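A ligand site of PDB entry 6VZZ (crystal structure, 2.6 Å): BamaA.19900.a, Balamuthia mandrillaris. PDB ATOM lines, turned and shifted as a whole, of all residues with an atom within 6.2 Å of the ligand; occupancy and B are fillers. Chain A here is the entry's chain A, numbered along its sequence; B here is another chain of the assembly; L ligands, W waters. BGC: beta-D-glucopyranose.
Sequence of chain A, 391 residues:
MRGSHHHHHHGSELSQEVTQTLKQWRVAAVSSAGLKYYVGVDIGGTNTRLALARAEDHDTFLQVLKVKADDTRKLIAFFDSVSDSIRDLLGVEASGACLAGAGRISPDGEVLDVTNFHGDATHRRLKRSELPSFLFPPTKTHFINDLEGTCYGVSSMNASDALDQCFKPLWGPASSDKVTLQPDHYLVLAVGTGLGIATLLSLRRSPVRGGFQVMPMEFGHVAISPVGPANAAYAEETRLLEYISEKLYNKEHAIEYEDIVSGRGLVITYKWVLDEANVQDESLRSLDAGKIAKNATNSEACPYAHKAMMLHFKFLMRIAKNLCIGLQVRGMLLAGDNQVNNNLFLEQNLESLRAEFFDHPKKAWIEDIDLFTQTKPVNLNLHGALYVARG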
ATOM      1  N   ILE A  43      -5.514   8.680  -9.541  1.00  0.00           N
ATOM      2  CA  ILE A  43      -4.943   9.896  -8.978  1.00  0.00           C
ATOM      3  C   ILE A  43      -3.457   9.648  -8.757  1.00  0.00           C
ATOM      4  O   ILE A  43      -3.063   8.988  -7.790  1.00  0.00           O
ATOM      5  CB  ILE A  43      -5.635  10.313  -7.683  1.00  0.00           C
ATOM      6  CG1 ILE A  43      -7.114  10.598  -7.930  1.00  0.00           C
ATOM      7  CG2 ILE A  43      -4.953  11.543  -7.116  1.00  0.00           C
ATOM      8  CD1 ILE A  43      -7.906  10.902  -6.658  1.00  0.00           C
ATOM      9  N   GLY A  44      -2.627  10.145  -9.678  1.00  0.00           N
ATOM     10  CA  GLY A  44      -1.191  10.068  -9.515  1.00  0.00           C
ATOM     11  C   GLY A  44      -0.619  11.279  -8.807  1.00  0.00           C
ATOM     12  O   GLY A  44      -1.305  12.258  -8.530  1.00  0.00           O
ATOM     13  N   GLY A  45       0.676  11.215  -8.514  1.00  0.00           N
ATOM     14  CA  GLY A  45       1.319  12.318  -7.841  1.00  0.00           C
ATOM     15  C   GLY A  45       1.458  13.563  -8.705  1.00  0.00           C
ATOM     16  O   GLY A  45       1.649  14.654  -8.166  1.00  0.00           O
ATOM     17  N   GLY A 101      -5.683   6.082  -5.757  1.00  0.00           N
ATOM     18  CA  GLY A 101      -4.827   7.229  -5.539  1.00  0.00           C
ATOM     19  C   GLY A 101      -3.447   6.900  -5.009  1.00  0.00           C
ATOM     20  O   GLY A 101      -3.257   5.865  -4.359  1.00  0.00           O
ATOM     21  N   ALA A 102      -2.487   7.785  -5.260  1.00  0.00           N
ATOM     22  CA  ALA A 102      -1.086   7.534  -4.932  1.00  0.00           C
ATOM     23  C   ALA A 102      -0.816   7.939  -3.482  1.00  0.00           C
ATOM     24  O   ALA A 102      -0.085   8.881  -3.178  1.00  0.00           O
ATOM     25  CB  ALA A 102      -0.174   8.272  -5.897  1.00  0.00           C
ATOM     26  N   GLY A 103      -1.435   7.209  -2.568  1.00  0.00           N
ATOM     27  CA  GLY A 103      -1.175   7.434  -1.166  1.00  0.00           C
ATOM     28  C   GLY A 103      -1.951   6.468  -0.302  1.00  0.00           C
ATOM     29  O   GLY A 103      -2.406   5.423  -0.769  1.00  0.00           O
ATOM     30  N   ARG A 104      -2.121   6.843   0.961  1.00  0.00           N
ATOM     31  CA  ARG A 104      -2.716   6.004   1.984  1.00  0.00           C
ATOM     32  C   ARG A 104      -4.175   6.354   2.160  1.00  0.00           C
ATOM     33  O   ARG A 104      -4.604   7.474   1.886  1.00  0.00           O
ATOM     34  CB  ARG A 104      -1.989   6.156   3.310  1.00  0.00           C
ATOM     35  CG  ARG A 104      -0.590   5.618   3.316  1.00  0.00           C
ATOM     36  CD  ARG A 104       0.347   6.575   3.996  1.00  0.00           C
ATOM     37  NE  ARG A 104       0.034   6.740   5.408  1.00  0.00           N
ATOM     38  CZ  ARG A 104      -0.273   7.909   5.976  1.00  0.00           C
ATOM     39  NH1 ARG A 104      -0.305   9.032   5.255  1.00  0.00           N
ATOM     40  NH2 ARG A 104      -0.534   7.952   7.270  1.00  0.00           N
ATOM     41  N   THR A 115       0.521  11.146  -1.144  1.00  0.00           N
ATOM     42  CA  THR A 115       1.797  11.293  -0.453  1.00  0.00           C
ATOM     43  C   THR A 115       2.615  12.452  -1.006  1.00  0.00           C
ATOM     44  O   THR A 115       3.266  13.179  -0.245  1.00  0.00           O
ATOM     45  CB  THR A 115       2.585   9.975  -0.557  1.00  0.00           C
ATOM     46  OG1 THR A 115       1.822   8.936   0.058  1.00  0.00           O
ATOM     47  CG2 THR A 115       3.945  10.096   0.135  1.00  0.00           C
ATOM     48  N   ASN A 116       2.608  12.647  -2.323  1.00  0.00           N
ATOM     49  CA  ASN A 116       3.533  13.572  -2.966  1.00  0.00           C
ATOM     50  C   ASN A 116       2.847  14.826  -3.496  1.00  0.00           C
ATOM     51  O   ASN A 116       3.440  15.562  -4.289  1.00  0.00           O
ATOM     52  CB  ASN A 116       4.304  12.857  -4.067  1.00  0.00           C
ATOM     53  CG  ASN A 116       5.390  11.926  -3.520  1.00  0.00           C
ATOM     54  OD1 ASN A 116       6.113  12.280  -2.595  1.00  0.00           O
ATOM     55  ND2 ASN A 116       5.493  10.742  -4.088  1.00  0.00           N
ATOM     56  N   ASN A 145      -5.584   2.225  -3.082  1.00  0.00           N
ATOM     57  CA  ASN A 145      -4.273   2.724  -3.469  1.00  0.00           C
ATOM     58  C   ASN A 145      -4.044   2.448  -4.950  1.00  0.00           C
ATOM     59  O   ASN A 145      -4.625   1.526  -5.532  1.00  0.00           O
ATOM     60  CB  ASN A 145      -3.202   2.066  -2.589  1.00  0.00           C
ATOM     61  CG  ASN A 145      -1.779   2.378  -3.040  1.00  0.00           C
ATOM     62  OD1 ASN A 145      -1.236   1.680  -3.891  1.00  0.00           O
ATOM     63  ND2 ASN A 145      -1.179   3.405  -2.450  1.00  0.00           N
ATOM     64  N   ASP A 146      -3.206   3.292  -5.578  1.00  0.00           N
ATOM     65  CA  ASP A 146      -3.006   3.163  -7.013  1.00  0.00           C
ATOM     66  C   ASP A 146      -2.360   1.831  -7.382  1.00  0.00           C
ATOM     67  O   ASP A 146      -2.795   1.171  -8.340  1.00  0.00           O
ATOM     68  CB  ASP A 146      -2.194   4.350  -7.558  1.00  0.00           C
ATOM     69  CG  ASP A 146      -0.839   4.515  -6.875  1.00  0.00           C
ATOM     70  OD1 ASP A 146      -0.640   3.990  -5.751  1.00  0.00           O
ATOM     71  OD2 ASP A 146       0.032   5.191  -7.468  1.00  0.00           O
ATOM     72  N   LEU A 147      -1.334   1.393  -6.643  1.00  0.00           N
ATOM     73  CA  LEU A 147      -0.740   0.095  -6.946  1.00  0.00           C
ATOM     74  C   LEU A 147      -1.689  -1.048  -6.587  1.00  0.00           C
ATOM     75  O   LEU A 147      -1.691  -2.090  -7.257  1.00  0.00           O
ATOM     76  CB  LEU A 147       0.592  -0.083  -6.221  1.00  0.00           C
ATOM     77  CG  LEU A 147       1.829   0.180  -7.091  1.00  0.00           C
ATOM     78  CD1 LEU A 147       1.999  -0.908  -8.131  1.00  0.00           C
ATOM     79  CD2 LEU A 147       1.720   1.532  -7.768  1.00  0.00           C
ATOM     80  N   ALA A 190       5.955  -0.068  -9.644  1.00  0.00           N
ATOM     81  CA  ALA A 190       5.784   0.933 -10.696  1.00  0.00           C
ATOM     82  C   ALA A 190       6.585   2.171 -10.328  1.00  0.00           C
ATOM     83  O   ALA A 190       6.417   2.722  -9.242  1.00  0.00           O
ATOM     84  CB  ALA A 190       4.309   1.299 -10.901  1.00  0.00           C
ATOM     85  N   THR A 193       6.000   9.202 -10.487  1.00  0.00           N
ATOM     86  CA  THR A 193       6.212  10.296  -9.542  1.00  0.00           C
ATOM     87  C   THR A 193       6.720   9.743  -8.211  1.00  0.00           C
ATOM     88  O   THR A 193       7.555  10.367  -7.552  1.00  0.00           O
ATOM     89  CB  THR A 193       4.923  11.095  -9.334  1.00  0.00           C
ATOM     90  OG1 THR A 193       4.378  11.461 -10.611  1.00  0.00           O
ATOM     91  CG2 THR A 193       5.201  12.359  -8.525  1.00  0.00           C
ATOM     92  N   GLY A 194       6.227   8.570  -7.819  1.00  0.00           N
ATOM     93  CA  GLY A 194       6.738   7.861  -6.661  1.00  0.00           C
ATOM     94  C   GLY A 194       7.111   6.437  -7.003  1.00  0.00           C
ATOM     95  O   GLY A 194       6.993   6.007  -8.157  1.00  0.00           O
ATOM     96  N   LEU A 195       7.587   5.719  -5.986  1.00  0.00           N
ATOM     97  CA  LEU A 195       7.841   4.284  -6.094  1.00  0.00           C
ATOM     98  C   LEU A 195       6.642   3.537  -5.520  1.00  0.00           C
ATOM     99  O   LEU A 195       6.429   3.526  -4.298  1.00  0.00           O
ATOM    100  CB  LEU A 195       9.124   3.903  -5.368  1.00  0.00           C
ATOM    101  CG  LEU A 195       9.467   2.407  -5.397  1.00  0.00           C
ATOM    102  CD1 LEU A 195       9.247   1.845  -6.789  1.00  0.00           C
ATOM    103  CD2 LEU A 195      10.904   2.178  -4.927  1.00  0.00           C
ATOM    104  N   GLY A 196       5.856   2.905  -6.392  1.00  0.00           N
ATOM    105  CA  GLY A 196       4.678   2.170  -5.984  1.00  0.00           C
ATOM    106  C   GLY A 196       4.977   0.680  -5.881  1.00  0.00           C
ATOM    107  O   GLY A 196       5.642   0.104  -6.748  1.00  0.00           O
ATOM    108  N   ILE A 197       4.452   0.062  -4.829  1.00  0.00           N
ATOM    109  CA  ILE A 197       4.695  -1.351  -4.559  1.00  0.00           C
ATOM    110  C   ILE A 197       3.450  -1.979  -3.931  1.00  0.00           C
ATOM    111  O   ILE A 197       2.921  -1.470  -2.932  1.00  0.00           O
ATOM    112  CB  ILE A 197       5.921  -1.545  -3.652  1.00  0.00           C
ATOM    113  CG1 ILE A 197       7.201  -1.193  -4.405  1.00  0.00           C
ATOM    114  CG2 ILE A 197       5.971  -2.979  -3.151  1.00  0.00           C
ATOM    115  CD1 ILE A 197       8.420  -1.266  -3.581  1.00  0.00           C
ATOM    116  N   MET A 217       0.849  -1.683  -0.225  1.00  0.00           N
ATOM    117  CA  MET A 217       2.099  -1.551   0.499  1.00  0.00           C
ATOM    118  C   MET A 217       2.684  -0.156   0.295  1.00  0.00           C
ATOM    119  O   MET A 217       2.309   0.583  -0.626  1.00  0.00           O
ATOM    120  CB  MET A 217       3.102  -2.622   0.066  1.00  0.00           C
ATOM    121  CG  MET A 217       2.693  -4.036   0.389  1.00  0.00           C
ATOM    122  SD  MET A 217       3.911  -5.251  -0.188  1.00  0.00           S
ATOM    123  CE  MET A 217       3.276  -6.744   0.587  1.00  0.00           C
ATOM    124  N   GLU A 218       3.642   0.210   1.157  1.00  0.00           N
ATOM    125  CA  GLU A 218       4.304   1.499   1.068  1.00  0.00           C
ATOM    126  C   GLU A 218       5.824   1.337   1.070  1.00  0.00           C
ATOM    127  O   GLU A 218       6.537   2.191   1.598  1.00  0.00           O
ATOM    128  CB  GLU A 218       3.862   2.403   2.209  1.00  0.00           C
ATOM    129  CG  GLU A 218       2.446   2.935   2.034  1.00  0.00           C
ATOM    130  CD  GLU A 218       2.330   3.871   0.851  1.00  0.00           C
ATOM    131  OE1 GLU A 218       3.370   4.486   0.454  1.00  0.00           O
ATOM    132  OE2 GLU A 218       1.215   3.988   0.289  1.00  0.00           O
ATOM    133  N   HIS A 221       9.034   3.820   0.560  1.00  0.00           N
ATOM    134  CA  HIS A 221       9.494   4.774   1.553  1.00  0.00           C
ATOM    135  C   HIS A 221      10.412   4.149   2.600  1.00  0.00           C
ATOM    136  O   HIS A 221      10.809   4.855   3.538  1.00  0.00           O
ATOM    137  CB  HIS A 221       8.283   5.444   2.200  1.00  0.00           C
ATOM    138  CG  HIS A 221       7.381   6.106   1.214  1.00  0.00           C
ATOM    139  ND1 HIS A 221       7.711   7.273   0.564  1.00  0.00           N
ATOM    140  CD2 HIS A 221       6.170   5.740   0.728  1.00  0.00           C
ATOM    141  CE1 HIS A 221       6.738   7.615  -0.257  1.00  0.00           C
ATOM    142  NE2 HIS A 221       5.792   6.693  -0.182  1.00  0.00           N
ATOM    143  N   GLU A 258      12.468   5.722  -2.721  1.00  0.00           N
ATOM    144  CA  GLU A 258      11.796   6.676  -3.604  1.00  0.00           C
ATOM    145  C   GLU A 258      12.614   7.951  -3.817  1.00  0.00           C
ATOM    146  O   GLU A 258      12.411   8.657  -4.805  1.00  0.00           O
ATOM    147  CB  GLU A 258      10.411   7.022  -3.050  1.00  0.00           C
ATOM    148  CG  GLU A 258       9.575   7.897  -3.994  1.00  0.00           C
ATOM    149  CD  GLU A 258       8.161   8.149  -3.483  1.00  0.00           C
ATOM    150  OE1 GLU A 258       7.368   7.189  -3.413  1.00  0.00           O
ATOM    151  OE2 GLU A 258       7.829   9.315  -3.148  1.00  0.00           O
ATOM    152  N   ARG A 264      11.705  12.641  -9.670  1.00  0.00           N
ATOM    153  CA  ARG A 264      12.576  13.589  -8.998  1.00  0.00           C
ATOM    154  C   ARG A 264      13.864  12.929  -8.530  1.00  0.00           C
ATOM    155  O   ARG A 264      14.905  13.578  -8.443  1.00  0.00           O
ATOM    156  CB  ARG A 264      11.841  14.253  -7.824  1.00  0.00           C
ATOM    157  CG  ARG A 264      11.566  13.353  -6.631  1.00  0.00           C
ATOM    158  CD  ARG A 264      10.591  13.996  -5.651  1.00  0.00           C
ATOM    159  NE  ARG A 264      10.419  13.175  -4.449  1.00  0.00           N
ATOM    160  CZ  ARG A 264       9.522  12.197  -4.336  1.00  0.00           C
ATOM    161  NH1 ARG A 264       8.703  11.919  -5.350  1.00  0.00           N
ATOM    162  NH2 ARG A 264       9.424  11.504  -3.204  1.00  0.00           N
ATOM    163  N   LYS B 362       9.217   9.550   7.364  1.00  0.00           N
ATOM    164  CA  LYS B 362       7.788   9.317   7.537  1.00  0.00           C
ATOM    165  C   LYS B 362       7.442   8.956   8.978  1.00  0.00           C
ATOM    166  O   LYS B 362       6.561   8.138   9.219  1.00  0.00           O
ATOM    167  CB  LYS B 362       7.317   8.202   6.601  1.00  0.00           C
ATOM    168  CG  LYS B 362       7.582   8.456   5.133  1.00  0.00           C
ATOM    169  CD  LYS B 362       6.820   9.670   4.632  1.00  0.00           C
ATOM    170  CE  LYS B 362       6.732   9.672   3.107  1.00  0.00           C
ATOM    171  NZ  LYS B 362       7.944  10.213   2.431  1.00  0.00           N
ATOM    172  N   TRP B 365       3.940   8.661  10.173  1.00  0.00           N
ATOM    173  CA  TRP B 365       3.115   7.503   9.804  1.00  0.00           C
ATOM    174  C   TRP B 365       3.133   6.411  10.863  1.00  0.00           C
ATOM    175  O   TRP B 365       2.180   5.644  10.961  1.00  0.00           O
ATOM    176  CB  TRP B 365       3.583   6.903   8.467  1.00  0.00           C
ATOM    177  CG  TRP B 365       3.390   7.760   7.276  1.00  0.00           C
ATOM    178  CD1 TRP B 365       3.016   9.069   7.262  1.00  0.00           C
ATOM    179  CD2 TRP B 365       3.549   7.373   5.907  1.00  0.00           C
ATOM    180  NE1 TRP B 365       2.943   9.521   5.968  1.00  0.00           N
ATOM    181  CE2 TRP B 365       3.266   8.502   5.117  1.00  0.00           C
ATOM    182  CE3 TRP B 365       3.901   6.171   5.281  1.00  0.00           C
ATOM    183  CZ2 TRP B 365       3.325   8.478   3.721  1.00  0.00           C
ATOM    184  CZ3 TRP B 365       3.960   6.147   3.884  1.00  0.00           C
ATOM    185  CH2 TRP B 365       3.673   7.296   3.124  1.00  0.00           C
HETATM  186  C2  BGC L   1       2.945   6.596  -2.344  1.00  0.00           C
HETATM  187  C3  BGC L   1       2.255   5.293  -2.692  1.00  0.00           C
HETATM  188  C4  BGC L   1       2.038   5.202  -4.192  1.00  0.00           C
HETATM  189  C5  BGC L   1       3.362   5.413  -4.914  1.00  0.00           C
HETATM  190  C6  BGC L   1       3.263   5.385  -6.419  1.00  0.00           C
HETATM  191  C1  BGC L   1       4.228   6.709  -3.144  1.00  0.00           C
HETATM  192  O1  BGC L   1       4.938   7.848  -2.803  1.00  0.00           O
HETATM  193  O2  BGC L   1       3.228   6.649  -0.943  1.00  0.00           O
HETATM  194  O3  BGC L   1       1.022   5.171  -1.995  1.00  0.00           O
HETATM  195  O4  BGC L   1       1.536   3.916  -4.545  1.00  0.00           O
HETATM  196  O5  BGC L   1       3.907   6.686  -4.532  1.00  0.00           O
HETATM  197  O6  BGC L   1       2.206   6.202  -6.887  1.00  0.00           O
HETATM  198  O   HOH W   1       2.590   1.774  -2.834  1.00  0.00           O
HETATM  199  O   HOH W   2       3.563   9.100  -5.713  1.00  0.00           O
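The side-chain carboxylate (OD2) of Asp 146 sits at hydrogen-bond distance from an oxygen (O6) of the ligand, 2.5 Å away.
OE1 of Glu 218 sits at hydrogen-bond distance from O2 of the ligand (2.6 Å).
An oxygen (O1) of the ligand is in hydrogen-bond range of the side-chain carboxylate (OE1) of Glu 258, at 2.6 Å.
An oxygen (O2) of the ligand is in hydrogen-bond range of a ring nitrogen (NE2) of His 221 (2.7 Å).
ND2 of Asn 145 sits at hydrogen-bond distance from O3 of the ligand (2.9 Å).
O2 of the ligand sits at hydrogen-bond distance from OG1 of Thr 115, 2.9 Å away.
The side-chain amide nitrogen of Asn 116 sits at hydrogen-bond distance from an oxygen (O1) of the ligand (3.2 Å).
The backbone NH of Gly 103 sits at hydrogen-bond distance from an oxygen (O3) of the ligand (3.2 Å).
OD1 of Asn 145 lies close to OD1 of Asp 146, at 3.0 Å.
The side-chain carboxylate (OE1) of Glu 218 sits close to a ring nitrogen (NE2) of His 221 (3.3 Å).
The side-chain carboxylate (OE2) of Glu 258 is in salt-bridge range of the guanidinium group (NH2) of Arg 264 (2.7 Å).
A ring nitrogen (ND1) of His 221 sits at hydrogen-bond distance from the side-chain amino group (NZ) of Lys 362 of chain B, 3.5 Å away.
N of Leu 147 is in hydrogen-bond range of OD1 of Asn 145 (2.8 Å).
The backbone NH of Thr 115 lies within hydrogen-bond range of the backbone carbonyl oxygen of Ala 102, 3.1 Å away.
OD1 of Asn 116 lies within hydrogen-bond range of NH2 of Arg 264 (3.5 Å).
The backbone NH (N) of Ala 102 sits at hydrogen-bond distance from the backbone carbonyl oxygen (O) of Ile 43 (2.9 Å).
Residues that only touch the ligand: Ala 102 (3.3 Å), Gly 194 (3.7 Å), Leu 195 (3.7 Å) and Gly 196 (3.5 Å).
Hydrophobic or aromatic side chains that line the ligand: Ala 102 and His 221.
Of the 25 residues printed, 12 come within 4 Å of the ligand.
Water W2 lies within hydrogen-bond range of O5 of the ligand (2.7 Å), ND2 of Asn 116 (3.0 Å) and N of Gly 194 (3.4 Å).
Water W1 lies within hydrogen-bond range of the backbone carbonyl oxygen of Met 217, an oxygen (O4) of the ligand and the backbone NH of Ile 197.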
